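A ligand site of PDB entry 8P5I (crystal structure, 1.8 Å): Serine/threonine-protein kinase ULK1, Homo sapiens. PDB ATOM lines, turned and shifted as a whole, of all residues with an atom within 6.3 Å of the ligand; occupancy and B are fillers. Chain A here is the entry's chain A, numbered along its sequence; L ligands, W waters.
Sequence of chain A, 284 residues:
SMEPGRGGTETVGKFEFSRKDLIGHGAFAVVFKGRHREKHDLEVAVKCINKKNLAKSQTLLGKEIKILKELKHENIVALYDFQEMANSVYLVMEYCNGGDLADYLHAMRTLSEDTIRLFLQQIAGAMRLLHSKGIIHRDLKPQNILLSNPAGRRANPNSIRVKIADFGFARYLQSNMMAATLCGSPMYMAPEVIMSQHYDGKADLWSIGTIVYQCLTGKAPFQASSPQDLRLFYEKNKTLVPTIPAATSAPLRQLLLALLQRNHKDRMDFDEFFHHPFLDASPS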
ATOM      1  N   ILE A  23      16.997  14.992   1.806  1.00  0.00           N
ATOM      2  CA  ILE A  23      17.166  15.291   3.236  1.00  0.00           C
ATOM      3  C   ILE A  23      18.550  14.894   3.760  1.00  0.00           C
ATOM      4  O   ILE A  23      18.874  15.209   4.887  1.00  0.00           O
ATOM      5  CB  ILE A  23      16.045  14.707   4.098  1.00  0.00           C
ATOM      6  CG1 ILE A  23      15.941  13.189   3.953  1.00  0.00           C
ATOM      7  CG2 ILE A  23      14.725  15.395   3.805  1.00  0.00           C
ATOM      8  CD1 ILE A  23      14.946  12.568   4.904  1.00  0.00           C
ATOM      9  N   GLY A  24      19.381  14.245   2.944  1.00  0.00           N
ATOM     10  CA  GLY A  24      20.743  13.963   3.349  1.00  0.00           C
ATOM     11  C   GLY A  24      21.570  13.431   2.204  1.00  0.00           C
ATOM     12  O   GLY A  24      21.044  12.792   1.274  1.00  0.00           O
ATOM     13  N   HIS A  25      22.864  13.699   2.254  1.00  0.00           N
ATOM     14  CA  HIS A  25      23.804  13.140   1.308  1.00  0.00           C
ATOM     15  C   HIS A  25      25.106  12.856   2.064  1.00  0.00           C
ATOM     16  O   HIS A  25      25.475  13.557   2.999  1.00  0.00           O
ATOM     17  CB  HIS A  25      23.948  14.041   0.077  1.00  0.00           C
ATOM     18  CG  HIS A  25      25.235  14.771  -0.042  1.00  0.00           C
ATOM     19  ND1 HIS A  25      25.544  15.930   0.638  1.00  0.00           N
ATOM     20  CD2 HIS A  25      26.318  14.469  -0.790  1.00  0.00           C
ATOM     21  CE1 HIS A  25      26.784  16.304   0.317  1.00  0.00           C
ATOM     22  NE2 HIS A  25      27.273  15.430  -0.549  1.00  0.00           N
ATOM     23  N   VAL A  31      19.568  10.397   0.678  1.00  0.00           N
ATOM     24  CA  VAL A  31      18.310  10.088   1.310  1.00  0.00           C
ATOM     25  C   VAL A  31      17.281  11.163   0.900  1.00  0.00           C
ATOM     26  O   VAL A  31      17.543  12.359   1.030  1.00  0.00           O
ATOM     27  CB  VAL A  31      18.475  10.075   2.829  1.00  0.00           C
ATOM     28  CG1 VAL A  31      17.194   9.687   3.540  1.00  0.00           C
ATOM     29  CG2 VAL A  31      19.626   9.160   3.248  1.00  0.00           C
ATOM     30  N   ALA A  45      11.632   7.745   4.624  1.00  0.00           N
ATOM     31  CA  ALA A  45      12.831   8.259   4.016  1.00  0.00           C
ATOM     32  C   ALA A  45      13.383   7.163   3.124  1.00  0.00           C
ATOM     33  O   ALA A  45      13.535   6.036   3.598  1.00  0.00           O
ATOM     34  CB  ALA A  45      13.860   8.569   5.116  1.00  0.00           C
ATOM     35  N   VAL A  46      13.723   7.494   1.890  1.00  0.00           N
ATOM     36  CA  VAL A  46      14.216   6.503   0.965  1.00  0.00           C
ATOM     37  C   VAL A  46      15.693   6.729   0.769  1.00  0.00           C
ATOM     38  O   VAL A  46      16.119   7.767   0.301  1.00  0.00           O
ATOM     39  CB  VAL A  46      13.470   6.548  -0.361  1.00  0.00           C
ATOM     40  CG1 VAL A  46      13.996   5.496  -1.324  1.00  0.00           C
ATOM     41  CG2 VAL A  46      11.984   6.387  -0.129  1.00  0.00           C
ATOM     42  N   LYS A  47      16.482   5.713   1.099  1.00  0.00           N
ATOM     43  CA  LYS A  47      17.913   5.792   0.909  1.00  0.00           C
ATOM     44  C   LYS A  47      18.307   5.093  -0.396  1.00  0.00           C
ATOM     45  O   LYS A  47      17.876   3.956  -0.634  1.00  0.00           O
ATOM     46  CB  LYS A  47      18.580   5.132   2.130  1.00  0.00           C
ATOM     47  CG  LYS A  47      20.081   5.289   2.126  1.00  0.00           C
ATOM     48  CD  LYS A  47      20.761   4.571   3.298  1.00  0.00           C
ATOM     49  CE  LYS A  47      20.630   5.302   4.597  1.00  0.00           C
ATOM     50  NZ  LYS A  47      21.705   4.935   5.572  1.00  0.00           N
ATOM     51  N   GLU A  64      23.556  -2.754   4.948  1.00  0.00           N
ATOM     52  CA  GLU A  64      22.572  -2.175   5.839  1.00  0.00           C
ATOM     53  C   GLU A  64      21.270  -2.965   5.777  1.00  0.00           C
ATOM     54  O   GLU A  64      20.636  -3.175   6.801  1.00  0.00           O
ATOM     55  CB  GLU A  64      22.404  -0.677   5.530  1.00  0.00           C
ATOM     56  CG  GLU A  64      21.438   0.014   6.468  1.00  0.00           C
ATOM     57  CD  GLU A  64      21.597   1.543   6.560  1.00  0.00           C
ATOM     58  OE1 GLU A  64      21.908   2.206   5.541  1.00  0.00           O
ATOM     59  OE2 GLU A  64      21.344   2.067   7.667  1.00  0.00           O
ATOM     60  N   VAL A  77      16.684   2.814  13.799  1.00  0.00           N
ATOM     61  CA  VAL A  77      15.949   3.242  12.619  1.00  0.00           C
ATOM     62  C   VAL A  77      15.293   2.033  11.951  1.00  0.00           C
ATOM     63  O   VAL A  77      15.935   1.010  11.731  1.00  0.00           O
ATOM     64  CB  VAL A  77      16.876   3.976  11.638  1.00  0.00           C
ATOM     65  CG1 VAL A  77      17.982   3.056  11.127  1.00  0.00           C
ATOM     66  CG2 VAL A  77      16.112   4.597  10.490  1.00  0.00           C
ATOM     67  N   ALA A  78      13.989   2.151  11.646  1.00  0.00           N
ATOM     68  CA  ALA A  78      13.237   1.053  11.083  1.00  0.00           C
ATOM     69  C   ALA A  78      13.461   0.986   9.578  1.00  0.00           C
ATOM     70  O   ALA A  78      13.701   1.967   8.897  1.00  0.00           O
ATOM     71  CB  ALA A  78      11.763   1.153  11.452  1.00  0.00           C
ATOM     72  N   MET A  93      12.864   3.548   4.746  1.00  0.00           N
ATOM     73  CA  MET A  93      13.252   3.646   6.150  1.00  0.00           C
ATOM     74  C   MET A  93      12.387   4.644   6.901  1.00  0.00           C
ATOM     75  O   MET A  93      11.677   5.481   6.335  1.00  0.00           O
ATOM     76  CB  MET A  93      14.729   4.075   6.212  1.00  0.00           C
ATOM     77  CG  MET A  93      15.631   3.224   5.377  1.00  0.00           C
ATOM     78  SD  MET A  93      17.378   3.448   5.670  1.00  0.00           S
ATOM     79  CE  MET A  93      17.429   2.466   7.154  1.00  0.00           C
ATOM     80  N   GLU A  94      12.465   4.526   8.227  1.00  0.00           N
ATOM     81  CA  GLU A  94      11.839   5.461   9.145  1.00  0.00           C
ATOM     82  C   GLU A  94      12.356   6.887   8.894  1.00  0.00           C
ATOM     83  O   GLU A  94      13.543   7.118   8.696  1.00  0.00           O
ATOM     84  CB  GLU A  94      12.178   5.050  10.561  1.00  0.00           C
ATOM     85  CG  GLU A  94      11.511   5.877  11.638  1.00  0.00           C
ATOM     86  CD  GLU A  94      11.863   5.383  13.017  1.00  0.00           C
ATOM     87  OE1 GLU A  94      12.582   4.327  13.142  1.00  0.00           O
ATOM     88  OE2 GLU A  94      11.428   6.043  13.995  1.00  0.00           O
ATOM     89  N   TYR A  95      11.417   7.824   8.841  1.00  0.00           N
ATOM     90  CA  TYR A  95      11.734   9.245   8.744  1.00  0.00           C
ATOM     91  C   TYR A  95      11.708   9.826  10.158  1.00  0.00           C
ATOM     92  O   TYR A  95      10.742   9.656  10.887  1.00  0.00           O
ATOM     93  CB  TYR A  95      10.684  10.007   7.891  1.00  0.00           C
ATOM     94  CG  TYR A  95      10.894  11.512   7.921  1.00  0.00           C
ATOM     95  CD1 TYR A  95      11.988  12.096   7.338  1.00  0.00           C
ATOM     96  CD2 TYR A  95       9.995  12.331   8.617  1.00  0.00           C
ATOM     97  CE1 TYR A  95      12.205  13.465   7.430  1.00  0.00           C
ATOM     98  CE2 TYR A  95      10.205  13.708   8.725  1.00  0.00           C
ATOM     99  CZ  TYR A  95      11.301  14.274   8.104  1.00  0.00           C
ATOM    100  OH  TYR A  95      11.589  15.630   8.174  1.00  0.00           O
ATOM    101  N   CYS A  96      12.864  10.329  10.582  1.00  0.00           N
ATOM    102  CA  CYS A  96      13.056  10.892  11.910  1.00  0.00           C
ATOM    103  C   CYS A  96      12.922  12.410  11.812  1.00  0.00           C
ATOM    104  O   CYS A  96      13.735  13.066  11.173  1.00  0.00           O
ATOM    105  CB  CYS A  96      14.420  10.460  12.442  1.00  0.00           C
ATOM    106  SG  CYS A  96      14.424   8.670  12.793  1.00  0.00           S
ATOM    107  N   ASN A  97      11.857  12.959  12.377  1.00  0.00           N
ATOM    108  CA  ASN A  97      11.493  14.351  12.070  1.00  0.00           C
ATOM    109  C   ASN A  97      12.327  15.407  12.802  1.00  0.00           C
ATOM    110  O   ASN A  97      12.219  16.589  12.453  1.00  0.00           O
ATOM    111  CB  ASN A  97      10.005  14.599  12.307  1.00  0.00           C
ATOM    112  CG  ASN A  97       9.601  14.457  13.753  1.00  0.00           C
ATOM    113  OD1 ASN A  97      10.425  14.321  14.639  1.00  0.00           O
ATOM    114  ND2 ASN A  97       8.315  14.541  14.034  1.00  0.00           N
ATOM    115  N   GLY A  98      13.228  14.987  13.712  1.00  0.00           N
ATOM    116  CA  GLY A  98      14.075  15.887  14.482  1.00  0.00           C
ATOM    117  C   GLY A  98      15.482  16.058  13.942  1.00  0.00           C
ATOM    118  O   GLY A  98      16.302  16.724  14.579  1.00  0.00           O
ATOM    119  N   GLY A  99      15.834  15.415  12.807  1.00  0.00           N
ATOM    120  CA  GLY A  99      17.179  15.466  12.264  1.00  0.00           C
ATOM    121  C   GLY A  99      18.169  14.681  13.162  1.00  0.00           C
ATOM    122  O   GLY A  99      17.776  13.745  13.847  1.00  0.00           O
ATOM    123  N   ASP A 100      19.417  15.113  13.204  1.00  0.00           N
ATOM    124  CA  ASP A 100      20.462  14.335  13.868  1.00  0.00           C
ATOM    125  C   ASP A 100      20.900  15.024  15.157  1.00  0.00           C
ATOM    126  O   ASP A 100      20.614  16.192  15.441  1.00  0.00           O
ATOM    127  CB  ASP A 100      21.599  14.068  12.897  1.00  0.00           C
ATOM    128  CG  ASP A 100      22.482  15.260  12.546  1.00  0.00           C
ATOM    129  OD1 ASP A 100      22.191  16.359  13.020  1.00  0.00           O
ATOM    130  OD2 ASP A 100      23.379  15.115  11.693  1.00  0.00           O
ATOM    131  N   GLN A 143      26.135  12.328  13.968  1.00  0.00           N
ATOM    132  CA  GLN A 143      25.481  12.401  12.669  1.00  0.00           C
ATOM    133  C   GLN A 143      24.616  11.130  12.449  1.00  0.00           C
ATOM    134  O   GLN A 143      23.678  11.122  11.647  1.00  0.00           O
ATOM    135  CB  GLN A 143      26.488  12.558  11.527  1.00  0.00           C
ATOM    136  CG  GLN A 143      27.293  13.861  11.545  1.00  0.00           C
ATOM    137  CD  GLN A 143      28.367  14.046  12.621  1.00  0.00           C
ATOM    138  OE1 GLN A 143      28.766  13.175  13.403  1.00  0.00           O
ATOM    139  NE2 GLN A 143      28.859  15.273  12.694  1.00  0.00           N
ATOM    140  N   ASN A 144      24.929  10.046  13.169  1.00  0.00           N
ATOM    141  CA  ASN A 144      24.252   8.746  12.989  1.00  0.00           C
ATOM    142  C   ASN A 144      23.336   8.428  14.147  1.00  0.00           C
ATOM    143  O   ASN A 144      22.859   7.293  14.301  1.00  0.00           O
ATOM    144  CB  ASN A 144      25.286   7.638  12.761  1.00  0.00           C
ATOM    145  CG  ASN A 144      25.880   7.698  11.396  1.00  0.00           C
ATOM    146  OD1 ASN A 144      25.333   8.354  10.512  1.00  0.00           O
ATOM    147  ND2 ASN A 144      27.008   7.035  11.186  1.00  0.00           N
ATOM    148  N   ILE A 145      23.053   9.423  14.996  1.00  0.00           N
ATOM    149  CA  ILE A 145      22.058   9.339  16.033  1.00  0.00           C
ATOM    150  C   ILE A 145      20.931  10.271  15.603  1.00  0.00           C
ATOM    151  O   ILE A 145      21.142  11.482  15.556  1.00  0.00           O
ATOM    152  CB  ILE A 145      22.599   9.756  17.414  1.00  0.00           C
ATOM    153  CG1 ILE A 145      23.846   8.973  17.844  1.00  0.00           C
ATOM    154  CG2 ILE A 145      21.519   9.710  18.476  1.00  0.00           C
ATOM    155  CD1 ILE A 145      23.616   7.502  17.957  1.00  0.00           C
ATOM    156  N   LEU A 146      19.766   9.736  15.301  1.00  0.00           N
ATOM    157  CA  LEU A 146      18.662  10.573  14.810  1.00  0.00           C
ATOM    158  C   LEU A 146      17.665  10.782  15.924  1.00  0.00           C
ATOM    159  O   LEU A 146      17.620  10.036  16.901  1.00  0.00           O
ATOM    160  CB  LEU A 146      17.997   9.935  13.597  1.00  0.00           C
ATOM    161  CG  LEU A 146      18.948   9.588  12.461  1.00  0.00           C
ATOM    162  CD1 LEU A 146      18.161   9.023  11.276  1.00  0.00           C
ATOM    163  CD2 LEU A 146      19.799  10.775  12.037  1.00  0.00           C
ATOM    164  N   LEU A 147      16.865  11.867  15.760  1.00  0.00           N
ATOM    165  CA  LEU A 147      15.896  12.255  16.758  1.00  0.00           C
ATOM    166  C   LEU A 147      14.509  12.385  16.116  1.00  0.00           C
ATOM    167  O   LEU A 147      14.367  12.780  14.957  1.00  0.00           O
ATOM    168  CB  LEU A 147      16.306  13.630  17.275  1.00  0.00           C
ATOM    169  CG  LEU A 147      17.751  13.834  17.732  1.00  0.00           C
ATOM    170  CD1 LEU A 147      17.913  15.258  18.257  1.00  0.00           C
ATOM    171  CD2 LEU A 147      18.102  12.849  18.819  1.00  0.00           C
ATOM    172  N   ALA A 165      21.246   4.995  13.702  1.00  0.00           N
ATOM    173  CA  ALA A 165      21.093   4.855  12.257  1.00  0.00           C
ATOM    174  C   ALA A 165      22.412   4.486  11.605  1.00  0.00           C
ATOM    175  O   ALA A 165      23.452   4.467  12.248  1.00  0.00           O
ATOM    176  CB  ALA A 165      20.523   6.120  11.678  1.00  0.00           C
ATOM    177  N   ASP A 166      22.371   4.298  10.272  1.00  0.00           N
ATOM    178  CA  ASP A 166      23.494   4.067   9.385  1.00  0.00           C
ATOM    179  C   ASP A 166      24.277   2.819   9.773  1.00  0.00           C
ATOM    180  O   ASP A 166      25.378   2.899  10.332  1.00  0.00           O
ATOM    181  CB  ASP A 166      24.498   5.198   9.231  1.00  0.00           C
ATOM    182  CG  ASP A 166      25.441   4.936   8.059  1.00  0.00           C
ATOM    183  OD1 ASP A 166      25.406   3.786   7.376  1.00  0.00           O
ATOM    184  OD2 ASP A 166      26.247   5.846   7.819  1.00  0.00           O
HETATM  185  C1  LIG L   1      19.331  11.740   6.137  1.00  0.00           C
HETATM  186  C2  LIG L   1      20.110   9.909   7.605  1.00  0.00           C
HETATM  187  C3  LIG L   1      21.190  10.672   8.054  1.00  0.00           C
HETATM  188  C4  LIG L   1      22.227  10.110   8.785  1.00  0.00           C
HETATM  189  C5  LIG L   1      22.238   8.760   9.019  1.00  0.00           C
HETATM  190  C6  LIG L   1      21.177   7.984   8.609  1.00  0.00           C
HETATM  191  C7  LIG L   1      19.044   7.592   7.412  1.00  0.00           C
HETATM  192  C8  LIG L   1      17.190   9.182   7.865  1.00  0.00           C
HETATM  193  C9  LIG L   1      15.996   9.225   8.538  1.00  0.00           C
HETATM  194  C10 LIG L   1      16.056  11.477   8.609  1.00  0.00           C
HETATM  195  C11 LIG L   1      15.089  15.082   9.112  1.00  0.00           C
HETATM  196  C12 LIG L   1      16.980  14.476   8.175  1.00  0.00           C
HETATM  197  C13 LIG L   1      15.039  18.035  10.239  1.00  0.00           C
HETATM  198  C14 LIG L   1      13.662  18.688  10.280  1.00  0.00           C
HETATM  199  C15 LIG L   1      14.416  18.019   7.760  1.00  0.00           C
HETATM  200  N1  LIG L   1      18.993  10.561   6.925  1.00  0.00           N
HETATM  201  C16 LIG L   1      20.073   8.544   7.934  1.00  0.00           C
HETATM  202  O1  LIG L   1      19.415   6.440   7.099  1.00  0.00           O
HETATM  203  N2  LIG L   1      17.728   7.943   7.406  1.00  0.00           N
HETATM  204  N3  LIG L   1      15.441  10.343   8.992  1.00  0.00           N
HETATM  205  N4  LIG L   1      17.223  11.556   7.958  1.00  0.00           N
HETATM  206  C17 LIG L   1      17.812  10.411   7.546  1.00  0.00           C
HETATM  207  N5  LIG L   1      15.453  12.651   9.048  1.00  0.00           N
HETATM  208  C18 LIG L   1      15.832  13.968   8.766  1.00  0.00           C
HETATM  209  N6  LIG L   1      15.775  16.165   8.727  1.00  0.00           N
HETATM  210  N7  LIG L   1      16.937  15.806   8.119  1.00  0.00           N
HETATM  211  C19 LIG L   1      15.444  17.610   8.820  1.00  0.00           C
HETATM  212  N8  LIG L   1      13.505  19.795   9.315  1.00  0.00           N
HETATM  213  C20 LIG L   1      13.937  19.459   7.947  1.00  0.00           C
HETATM  214  C21 LIG L   1      16.743   6.933   6.959  1.00  0.00           C
HETATM  215  O   HOH W   1      20.165   4.191   8.589  1.00  0.00           O
HETATM  216  O   HOH W   2      23.012  13.124   9.959  1.00  0.00           O
HETATM  217  O   HOH W   3      17.662  17.582   6.199  1.00  0.00           O
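The side-chain amino group of Lys 47 is in salt-bridge range of the side-chain carboxylate of Glu 64 (2.7 Å). O of Ala 78 sits at hydrogen-bond distance from N of Glu 94, at 2.9 Å. N of Ala 165 sits at hydrogen-bond distance from O of Asn 144 (2.9 Å). The backbone carbonyl oxygen (O) of Ala 45 lies within hydrogen-bond range of the backbone NH (N) of Met 93. The backbone carbonyl oxygen (O) of Val 31 sits at hydrogen-bond distance from the backbone NH (N) of Ile 23, at 2.8 Å. O of Gly 99 is in hydrogen-bond range of N of Leu 147 (2.8 Å). N of Val 31 sits at hydrogen-bond distance from O of Gly 24.
O of Ile 23 touches C1 of the ligand, 3.7 Å away. Gly 24 touches the ligand (CA to C1, 3.8 Å). CB of Val 31 touches C1 of the ligand, at 3.8 Å. CB of Ala 45 touches C21 of the ligand (3.8 Å). Met 93 touches the ligand. Glu 94 touches the ligand. Tyr 95 touches the ligand. Asn 97 touches the ligand. Gly 99 touches the ligand. O of Gln 143 touches C4 of the ligand (3.4 Å). Asn 144 touches the ligand. Leu 146 touches the ligand. CB of Ala 165 touches C6 of the ligand, at 3.6 Å. 15 residues have an atom within 4 Å of the ligand: Ile 23, Gly 24, Val 31, Ala 45, Lys 47, Met 93, Glu 94, Tyr 95, Cys 96, Asn 97, Gly 99, Gln 143, Asn 144, Leu 146 and Ala 165. The nearest printed residue that does not touch the ligand is Asp 166 (4.2 Å).
A nitrogen (N3) of the ligand sits at hydrogen-bond distance from the backbone NH (N) of Cys 96. The backbone carbonyl oxygen (O) of Cys 96 sits at hydrogen-bond distance from a nitrogen (N5) of the ligand (2.8 Å). NZ of Lys 47 sits close to O1 of the ligand (3.1 Å).
Water W3 bridges a nitrogen (N7) of the ligand and the backbone carbonyl oxygen of Ile 23. Water W1 lies within hydrogen-bond range of OE2 of Glu 64 (2.6 Å), N of Asp 166 (2.8 Å), O1 of the ligand (2.8 Å) and NZ of Lys 47 (3.5 Å). Water W2 bridges OD2 of Asp 100 (2.7 Å) and O of Gln 143 (2.7 Å).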
